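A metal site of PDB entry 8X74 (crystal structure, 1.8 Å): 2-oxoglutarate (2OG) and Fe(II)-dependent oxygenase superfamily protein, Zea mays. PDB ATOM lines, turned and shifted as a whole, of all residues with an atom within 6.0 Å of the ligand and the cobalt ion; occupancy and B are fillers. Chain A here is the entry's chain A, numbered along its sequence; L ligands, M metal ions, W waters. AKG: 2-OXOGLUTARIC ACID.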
ATOM      1  N   GLN A 138     -15.450  25.230 -17.112  1.00  0.00           N
ATOM      2  CA  GLN A 138     -16.278  24.839 -15.980  1.00  0.00           C
ATOM      3  C   GLN A 138     -15.568  23.782 -15.144  1.00  0.00           C
ATOM      4  O   GLN A 138     -14.700  23.050 -15.639  1.00  0.00           O
ATOM      5  CB  GLN A 138     -17.649  24.292 -16.424  1.00  0.00           C
ATOM      6  CG  GLN A 138     -17.618  22.827 -16.934  1.00  0.00           C
ATOM      7  CD  GLN A 138     -18.968  22.114 -16.761  1.00  0.00           C
ATOM      8  OE1 GLN A 138     -19.439  21.398 -17.645  1.00  0.00           O
ATOM      9  NE2 GLN A 138     -19.595  22.313 -15.624  1.00  0.00           N
ATOM     10  N   ARG A 209     -25.336  16.527 -10.890  1.00  0.00           N
ATOM     11  CA  ARG A 209     -24.162  17.221 -11.411  1.00  0.00           C
ATOM     12  C   ARG A 209     -24.282  18.696 -11.056  1.00  0.00           C
ATOM     13  O   ARG A 209     -25.161  19.394 -11.577  1.00  0.00           O
ATOM     14  CB  ARG A 209     -24.013  17.019 -12.911  1.00  0.00           C
ATOM     15  CG  ARG A 209     -22.852  17.814 -13.532  1.00  0.00           C
ATOM     16  CD  ARG A 209     -22.748  17.492 -15.021  1.00  0.00           C
ATOM     17  NE  ARG A 209     -21.689  18.276 -15.676  1.00  0.00           N
ATOM     18  CZ  ARG A 209     -20.594  17.751 -16.240  1.00  0.00           C
ATOM     19  NH1 ARG A 209     -20.369  16.450 -16.220  1.00  0.00           N
ATOM     20  NH2 ARG A 209     -19.699  18.557 -16.811  1.00  0.00           N
ATOM     21  N   ASN A 211     -22.696  22.082 -11.591  1.00  0.00           N
ATOM     22  CA  ASN A 211     -21.808  22.780 -12.523  1.00  0.00           C
ATOM     23  C   ASN A 211     -21.416  24.124 -11.957  1.00  0.00           C
ATOM     24  O   ASN A 211     -22.263  24.868 -11.466  1.00  0.00           O
ATOM     25  CB  ASN A 211     -22.495  22.984 -13.871  1.00  0.00           C
ATOM     26  CG  ASN A 211     -22.851  21.691 -14.545  1.00  0.00           C
ATOM     27  OD1 ASN A 211     -21.973  20.914 -14.906  1.00  0.00           O
ATOM     28  ND2 ASN A 211     -24.141  21.464 -14.738  1.00  0.00           N
ATOM     29  N   TYR A 213     -19.452  27.467 -13.396  1.00  0.00           N
ATOM     30  CA  TYR A 213     -18.838  28.154 -14.528  1.00  0.00           C
ATOM     31  C   TYR A 213     -18.215  29.447 -14.042  1.00  0.00           C
ATOM     32  O   TYR A 213     -18.947  30.400 -13.748  1.00  0.00           O
ATOM     33  CB  TYR A 213     -19.863  28.452 -15.623  1.00  0.00           C
ATOM     34  CG  TYR A 213     -20.700  27.260 -16.050  1.00  0.00           C
ATOM     35  CD1 TYR A 213     -21.883  26.972 -15.390  1.00  0.00           C
ATOM     36  CD2 TYR A 213     -20.309  26.457 -17.134  1.00  0.00           C
ATOM     37  CE1 TYR A 213     -22.658  25.874 -15.773  1.00  0.00           C
ATOM     38  CE2 TYR A 213     -21.090  25.352 -17.520  1.00  0.00           C
ATOM     39  CZ  TYR A 213     -22.248  25.076 -16.842  1.00  0.00           C
ATOM     40  OH  TYR A 213     -23.011  23.992 -17.218  1.00  0.00           O
ATOM     41  N   ILE A 225     -20.139  24.768 -21.147  1.00  0.00           N
ATOM     42  CA  ILE A 225     -20.192  23.339 -21.419  1.00  0.00           C
ATOM     43  C   ILE A 225     -20.494  23.181 -22.913  1.00  0.00           C
ATOM     44  O   ILE A 225     -21.322  23.907 -23.463  1.00  0.00           O
ATOM     45  CB  ILE A 225     -21.226  22.587 -20.531  1.00  0.00           C
ATOM     46  CG1 ILE A 225     -20.964  21.087 -20.614  1.00  0.00           C
ATOM     47  CG2 ILE A 225     -22.664  22.928 -20.887  1.00  0.00           C
ATOM     48  CD1 ILE A 225     -21.769  20.251 -19.592  1.00  0.00           C
ATOM     49  N   HIS A 228     -23.979  19.306 -26.485  1.00  0.00           N
ATOM     50  CA  HIS A 228     -24.140  17.905 -26.155  1.00  0.00           C
ATOM     51  C   HIS A 228     -25.620  17.635 -25.946  1.00  0.00           C
ATOM     52  O   HIS A 228     -26.411  18.564 -25.731  1.00  0.00           O
ATOM     53  CB  HIS A 228     -23.354  17.545 -24.876  1.00  0.00           C
ATOM     54  CG  HIS A 228     -23.947  18.134 -23.637  1.00  0.00           C
ATOM     55  ND1 HIS A 228     -23.774  19.447 -23.296  1.00  0.00           N
ATOM     56  CD2 HIS A 228     -24.735  17.592 -22.685  1.00  0.00           C
ATOM     57  CE1 HIS A 228     -24.428  19.701 -22.171  1.00  0.00           C
ATOM     58  NE2 HIS A 228     -25.026  18.595 -21.781  1.00  0.00           N
ATOM     59  N   SER A 229     -25.997  16.374 -26.030  1.00  0.00           N
ATOM     60  CA  SER A 229     -27.276  15.931 -25.487  1.00  0.00           C
ATOM     61  C   SER A 229     -27.018  15.060 -24.258  1.00  0.00           C
ATOM     62  O   SER A 229     -25.960  14.427 -24.141  1.00  0.00           O
ATOM     63  CB  SER A 229     -28.125  15.182 -26.522  1.00  0.00           C
ATOM     64  OG  SER A 229     -27.419  14.080 -27.088  1.00  0.00           O
ATOM     65  N   ASP A 230     -27.962  15.065 -23.325  1.00  0.00           N
ATOM     66  CA  ASP A 230     -27.765  14.258 -22.128  1.00  0.00           C
ATOM     67  C   ASP A 230     -28.097  12.795 -22.436  1.00  0.00           C
ATOM     68  O   ASP A 230     -28.840  12.484 -23.364  1.00  0.00           O
ATOM     69  CB  ASP A 230     -28.676  14.724 -20.987  1.00  0.00           C
ATOM     70  CG  ASP A 230     -28.443  16.140 -20.587  1.00  0.00           C
ATOM     71  OD1 ASP A 230     -27.336  16.664 -20.815  1.00  0.00           O
ATOM     72  OD2 ASP A 230     -29.369  16.726 -20.006  1.00  0.00           O
ATOM     73  N   THR A 235     -33.768  15.022 -17.827  1.00  0.00           N
ATOM     74  CA  THR A 235     -32.904  15.808 -16.949  1.00  0.00           C
ATOM     75  C   THR A 235     -33.763  16.912 -16.361  1.00  0.00           C
ATOM     76  O   THR A 235     -34.533  17.563 -17.079  1.00  0.00           O
ATOM     77  CB  THR A 235     -31.730  16.423 -17.732  1.00  0.00           C
ATOM     78  OG1 THR A 235     -30.950  15.383 -18.321  1.00  0.00           O
ATOM     79  CG2 THR A 235     -30.850  17.323 -16.859  1.00  0.00           C
ATOM     80  N   LEU A 237     -33.263  20.417 -14.434  1.00  0.00           N
ATOM     81  CA  LEU A 237     -32.160  21.370 -14.295  1.00  0.00           C
ATOM     82  C   LEU A 237     -32.593  22.571 -13.481  1.00  0.00           C
ATOM     83  O   LEU A 237     -33.644  23.167 -13.733  1.00  0.00           O
ATOM     84  CB  LEU A 237     -31.692  21.855 -15.677  1.00  0.00           C
ATOM     85  CG  LEU A 237     -30.573  22.893 -15.740  1.00  0.00           C
ATOM     86  CD1 LEU A 237     -29.185  22.275 -15.407  1.00  0.00           C
ATOM     87  CD2 LEU A 237     -30.550  23.534 -17.100  1.00  0.00           C
ATOM     88  N   VAL A 239     -31.054  26.346 -12.363  1.00  0.00           N
ATOM     89  CA  VAL A 239     -30.007  27.341 -12.614  1.00  0.00           C
ATOM     90  C   VAL A 239     -30.091  28.384 -11.514  1.00  0.00           C
ATOM     91  O   VAL A 239     -31.138  29.031 -11.341  1.00  0.00           O
ATOM     92  CB  VAL A 239     -30.130  27.978 -14.008  1.00  0.00           C
ATOM     93  CG1 VAL A 239     -29.066  29.070 -14.205  1.00  0.00           C
ATOM     94  CG2 VAL A 239     -29.995  26.914 -15.091  1.00  0.00           C
ATOM     95  N   GLY A 245     -27.082  31.805 -19.940  1.00  0.00           N
ATOM     96  CA  GLY A 245     -25.974  31.026 -20.481  1.00  0.00           C
ATOM     97  C   GLY A 245     -26.428  29.790 -21.224  1.00  0.00           C
ATOM     98  O   GLY A 245     -25.796  29.368 -22.193  1.00  0.00           O
ATOM     99  N   LEU A 246     -27.528  29.206 -20.771  1.00  0.00           N
ATOM    100  CA  LEU A 246     -28.014  27.970 -21.375  1.00  0.00           C
ATOM    101  C   LEU A 246     -28.639  28.267 -22.734  1.00  0.00           C
ATOM    102  O   LEU A 246     -29.421  29.198 -22.877  1.00  0.00           O
ATOM    103  CB  LEU A 246     -29.039  27.296 -20.464  1.00  0.00           C
ATOM    104  CG  LEU A 246     -29.654  26.030 -21.048  1.00  0.00           C
ATOM    105  CD1 LEU A 246     -28.595  24.945 -21.243  1.00  0.00           C
ATOM    106  CD2 LEU A 246     -30.780  25.548 -20.139  1.00  0.00           C
ATOM    107  N   ASN A 267     -35.550  18.513 -19.758  1.00  0.00           N
ATOM    108  CA  ASN A 267     -35.209  18.192 -21.132  1.00  0.00           C
ATOM    109  C   ASN A 267     -35.062  16.683 -21.260  1.00  0.00           C
ATOM    110  O   ASN A 267     -34.784  15.978 -20.296  1.00  0.00           O
ATOM    111  CB  ASN A 267     -33.913  18.927 -21.626  1.00  0.00           C
ATOM    112  CG  ASN A 267     -32.632  18.520 -20.874  1.00  0.00           C
ATOM    113  OD1 ASN A 267     -32.246  19.174 -19.893  1.00  0.00           O
ATOM    114  ND2 ASN A 267     -31.953  17.495 -21.355  1.00  0.00           N
ATOM    115  N   HIS A 285     -27.679  20.964 -26.432  1.00  0.00           N
ATOM    116  CA  HIS A 285     -27.659  22.212 -25.673  1.00  0.00           C
ATOM    117  C   HIS A 285     -26.234  22.505 -25.245  1.00  0.00           C
ATOM    118  O   HIS A 285     -25.352  21.645 -25.271  1.00  0.00           O
ATOM    119  CB  HIS A 285     -28.632  22.155 -24.453  1.00  0.00           C
ATOM    120  CG  HIS A 285     -28.436  20.963 -23.561  1.00  0.00           C
ATOM    121  ND1 HIS A 285     -28.874  19.697 -23.902  1.00  0.00           N
ATOM    122  CD2 HIS A 285     -27.819  20.827 -22.352  1.00  0.00           C
ATOM    123  CE1 HIS A 285     -28.532  18.840 -22.955  1.00  0.00           C
ATOM    124  NE2 HIS A 285     -27.898  19.502 -22.005  1.00  0.00           N
ATOM    125  N   ARG A 286     -26.003  23.759 -24.848  1.00  0.00           N
ATOM    126  CA  ARG A 286     -24.670  24.197 -24.453  1.00  0.00           C
ATOM    127  C   ARG A 286     -24.829  25.351 -23.486  1.00  0.00           C
ATOM    128  O   ARG A 286     -25.912  25.925 -23.357  1.00  0.00           O
ATOM    129  CB  ARG A 286     -23.835  24.623 -25.668  1.00  0.00           C
ATOM    130  CG  ARG A 286     -24.371  25.888 -26.316  1.00  0.00           C
ATOM    131  CD  ARG A 286     -23.593  26.253 -27.594  1.00  0.00           C
ATOM    132  NE  ARG A 286     -23.971  27.592 -28.035  1.00  0.00           N
ATOM    133  CZ  ARG A 286     -23.588  28.133 -29.192  1.00  0.00           C
ATOM    134  NH1 ARG A 286     -22.811  27.451 -30.032  1.00  0.00           N
ATOM    135  NH2 ARG A 286     -23.980  29.361 -29.517  1.00  0.00           N
ATOM    136  N   VAL A 287     -23.723  25.717 -22.822  1.00  0.00           N
ATOM    137  CA  VAL A 287     -23.685  26.909 -21.977  1.00  0.00           C
ATOM    138  C   VAL A 287     -22.576  27.818 -22.466  1.00  0.00           C
ATOM    139  O   VAL A 287     -21.441  27.362 -22.671  1.00  0.00           O
ATOM    140  CB  VAL A 287     -23.480  26.574 -20.492  1.00  0.00           C
ATOM    141  CG1 VAL A 287     -23.350  27.852 -19.668  1.00  0.00           C
ATOM    142  CG2 VAL A 287     -24.662  25.765 -19.977  1.00  0.00           C
ATOM    143  N   ARG A 295     -21.492  31.278 -12.784  1.00  0.00           N
ATOM    144  CA  ARG A 295     -22.830  30.715 -12.971  1.00  0.00           C
ATOM    145  C   ARG A 295     -22.842  29.307 -12.393  1.00  0.00           C
ATOM    146  O   ARG A 295     -21.872  28.562 -12.549  1.00  0.00           O
ATOM    147  CB  ARG A 295     -23.213  30.685 -14.450  1.00  0.00           C
ATOM    148  CG  ARG A 295     -24.568  30.053 -14.777  1.00  0.00           C
ATOM    149  CD  ARG A 295     -24.774  30.077 -16.296  1.00  0.00           C
ATOM    150  NE  ARG A 295     -26.079  29.538 -16.699  1.00  0.00           N
ATOM    151  CZ  ARG A 295     -26.345  28.240 -16.834  1.00  0.00           C
ATOM    152  NH1 ARG A 295     -25.424  27.323 -16.609  1.00  0.00           N
ATOM    153  NH2 ARG A 295     -27.559  27.860 -17.206  1.00  0.00           N
ATOM    154  N   LEU A 296     -23.938  28.945 -11.726  1.00  0.00           N
ATOM    155  CA  LEU A 296     -24.042  27.633 -11.081  1.00  0.00           C
ATOM    156  C   LEU A 296     -25.350  26.980 -11.468  1.00  0.00           C
ATOM    157  O   LEU A 296     -26.390  27.639 -11.528  1.00  0.00           O
ATOM    158  CB  LEU A 296     -23.988  27.724  -9.547  1.00  0.00           C
ATOM    159  CG  LEU A 296     -22.706  28.130  -8.832  1.00  0.00           C
ATOM    160  CD1 LEU A 296     -22.547  29.640  -8.844  1.00  0.00           C
ATOM    161  CD2 LEU A 296     -22.754  27.628  -7.404  1.00  0.00           C
ATOM    162  N   SER A 297     -25.284  25.682 -11.730  1.00  0.00           N
ATOM    163  CA  SER A 297     -26.492  24.929 -12.021  1.00  0.00           C
ATOM    164  C   SER A 297     -26.385  23.553 -11.398  1.00  0.00           C
ATOM    165  O   SER A 297     -25.293  23.054 -11.103  1.00  0.00           O
ATOM    166  CB  SER A 297     -26.741  24.812 -13.516  1.00  0.00           C
ATOM    167  OG  SER A 297     -25.767  23.968 -14.126  1.00  0.00           O
ATOM    168  N   ALA A 299     -27.907  19.818 -12.400  1.00  0.00           N
ATOM    169  CA  ALA A 299     -28.635  18.908 -13.276  1.00  0.00           C
ATOM    170  C   ALA A 299     -28.866  17.599 -12.542  1.00  0.00           C
ATOM    171  O   ALA A 299     -27.917  16.988 -12.033  1.00  0.00           O
ATOM    172  CB  ALA A 299     -27.842  18.677 -14.567  1.00  0.00           C
ATOM    173  N   PHE A 301     -29.886  14.077 -13.513  1.00  0.00           N
ATOM    174  CA  PHE A 301     -30.052  13.162 -14.633  1.00  0.00           C
ATOM    175  C   PHE A 301     -30.797  11.925 -14.157  1.00  0.00           C
ATOM    176  O   PHE A 301     -30.330  11.257 -13.240  1.00  0.00           O
ATOM    177  CB  PHE A 301     -28.701  12.744 -15.219  1.00  0.00           C
ATOM    178  CG  PHE A 301     -27.831  13.893 -15.636  1.00  0.00           C
ATOM    179  CD1 PHE A 301     -28.200  14.724 -16.683  1.00  0.00           C
ATOM    180  CD2 PHE A 301     -26.634  14.126 -14.989  1.00  0.00           C
ATOM    181  CE1 PHE A 301     -27.374  15.782 -17.065  1.00  0.00           C
ATOM    182  CE2 PHE A 301     -25.816  15.189 -15.369  1.00  0.00           C
ATOM    183  CZ  PHE A 301     -26.178  16.011 -16.409  1.00  0.00           C
HETATM  184  C1  AKG L   1     -25.383  19.347 -18.016  1.00  0.00           C
HETATM  185  O1  AKG L   1     -24.886  19.357 -16.853  1.00  0.00           O
HETATM  186  O2  AKG L   1     -25.492  18.291 -18.712  1.00  0.00           O
HETATM  187  C2  AKG L   1     -25.842  20.666 -18.591  1.00  0.00           C
HETATM  188  O5  AKG L   1     -26.118  20.728 -19.762  1.00  0.00           O
HETATM  189  C3  AKG L   1     -25.946  21.876 -17.662  1.00  0.00           C
HETATM  190  C4  AKG L   1     -26.630  23.026 -18.391  1.00  0.00           C
HETATM  191  C5  AKG L   1     -26.594  24.284 -17.539  1.00  0.00           C
HETATM  192  O3  AKG L   1     -25.623  24.502 -16.742  1.00  0.00           O
HETATM  193  O4  AKG L   1     -27.517  25.116 -17.670  1.00  0.00           O
HETATM  194 CO    CO M   1     -26.677  18.683 -20.442  1.00  0.00          CO
HETATM  195  O   HOH W   1     -28.332  18.975 -19.094  1.00  0.00           O
HETATM  196  O   HOH W   2     -24.671  15.134 -19.955  1.00  0.00           O
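The backbone carbonyl oxygen (O) of Ser 297 sits at hydrogen-bond distance from the backbone NH (N) of Asn 211, 2.8 Å away. The backbone NH of Tyr 213 sits at hydrogen-bond distance from the backbone carbonyl oxygen of Arg 295 (2.8 Å). The side-chain hydroxyl (OG1) of Thr 235 lies within hydrogen-bond range of the side-chain carboxylate (OD2) of Asp 230 (2.7 Å). OD1 of Asn 211 sits at hydrogen-bond distance from NE2 of Gln 138. N of Arg 209 sits at hydrogen-bond distance from O of Ala 299, at 2.9 Å. The side-chain amide oxygen (OD1) of Asn 211 is in hydrogen-bond range of the guanidinium group (NE) of Arg 209, 2.8 Å away. O of Ile 225 is in hydrogen-bond range of N of Val 287, at 3.1 Å. The side-chain carboxylate (OD2) of Asp 230 lies within hydrogen-bond range of the side-chain amide nitrogen (ND2) of Asn 267, 3.0 Å away.
CD2 of Leu 237 touches O4 of the ligand, at 3.5 Å. Leu 246 touches the ligand (CD1 to O4, 3.7 Å). Val 287 touches the ligand (CG2 to C5, 3.4 Å). Ala 299 touches the ligand. Phe 301 touches the ligand. Hydrophobic or aromatic side chains that line the ligand: Tyr 213, His 228, Leu 237, Leu 246, His 285, Val 287, Ala 299 and Phe 301. Of the 22 residues printed, 13 come within 4 Å of the ligand. Along chain A the residues within 4 Å of the ligand span positions 209 to 301.
Of the 22 residues printed, 3 come within 4 Å of the cobalt ion. The nearest printed residue that does not touch the cobalt ion is Phe 301 (4.5 Å).
The cobalt ion is bound by a ring nitrogen (NE2) of His 228 (2.1 Å), an oxygen (O2) of the ligand (2.1 Å), a ring nitrogen (NE2) of His 285 (2.1 Å), water W1 (2.2 Å), the side-chain carboxylate of Asp 230 (2.2 Å) and an oxygen (O5) of the ligand (2.2 Å).
The guanidinium group (NH2) of Arg 295 is in salt-bridge range of an oxygen (O4) of the ligand (2.8 Å). The side-chain hydroxyl (OG) of Ser 297 lies within hydrogen-bond range of an oxygen (O3) of the ligand (2.7 Å). The guanidinium group of Arg 209 is in salt-bridge range of an oxygen (O1) of the ligand, 3.6 Å away. An oxygen (O1) of the ligand is in hydrogen-bond range of the side-chain amide nitrogen (ND2) of Asn 211, 3.1 Å away. The side-chain hydroxyl (OH) of Tyr 213 sits at hydrogen-bond distance from an oxygen (O3) of the ligand.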
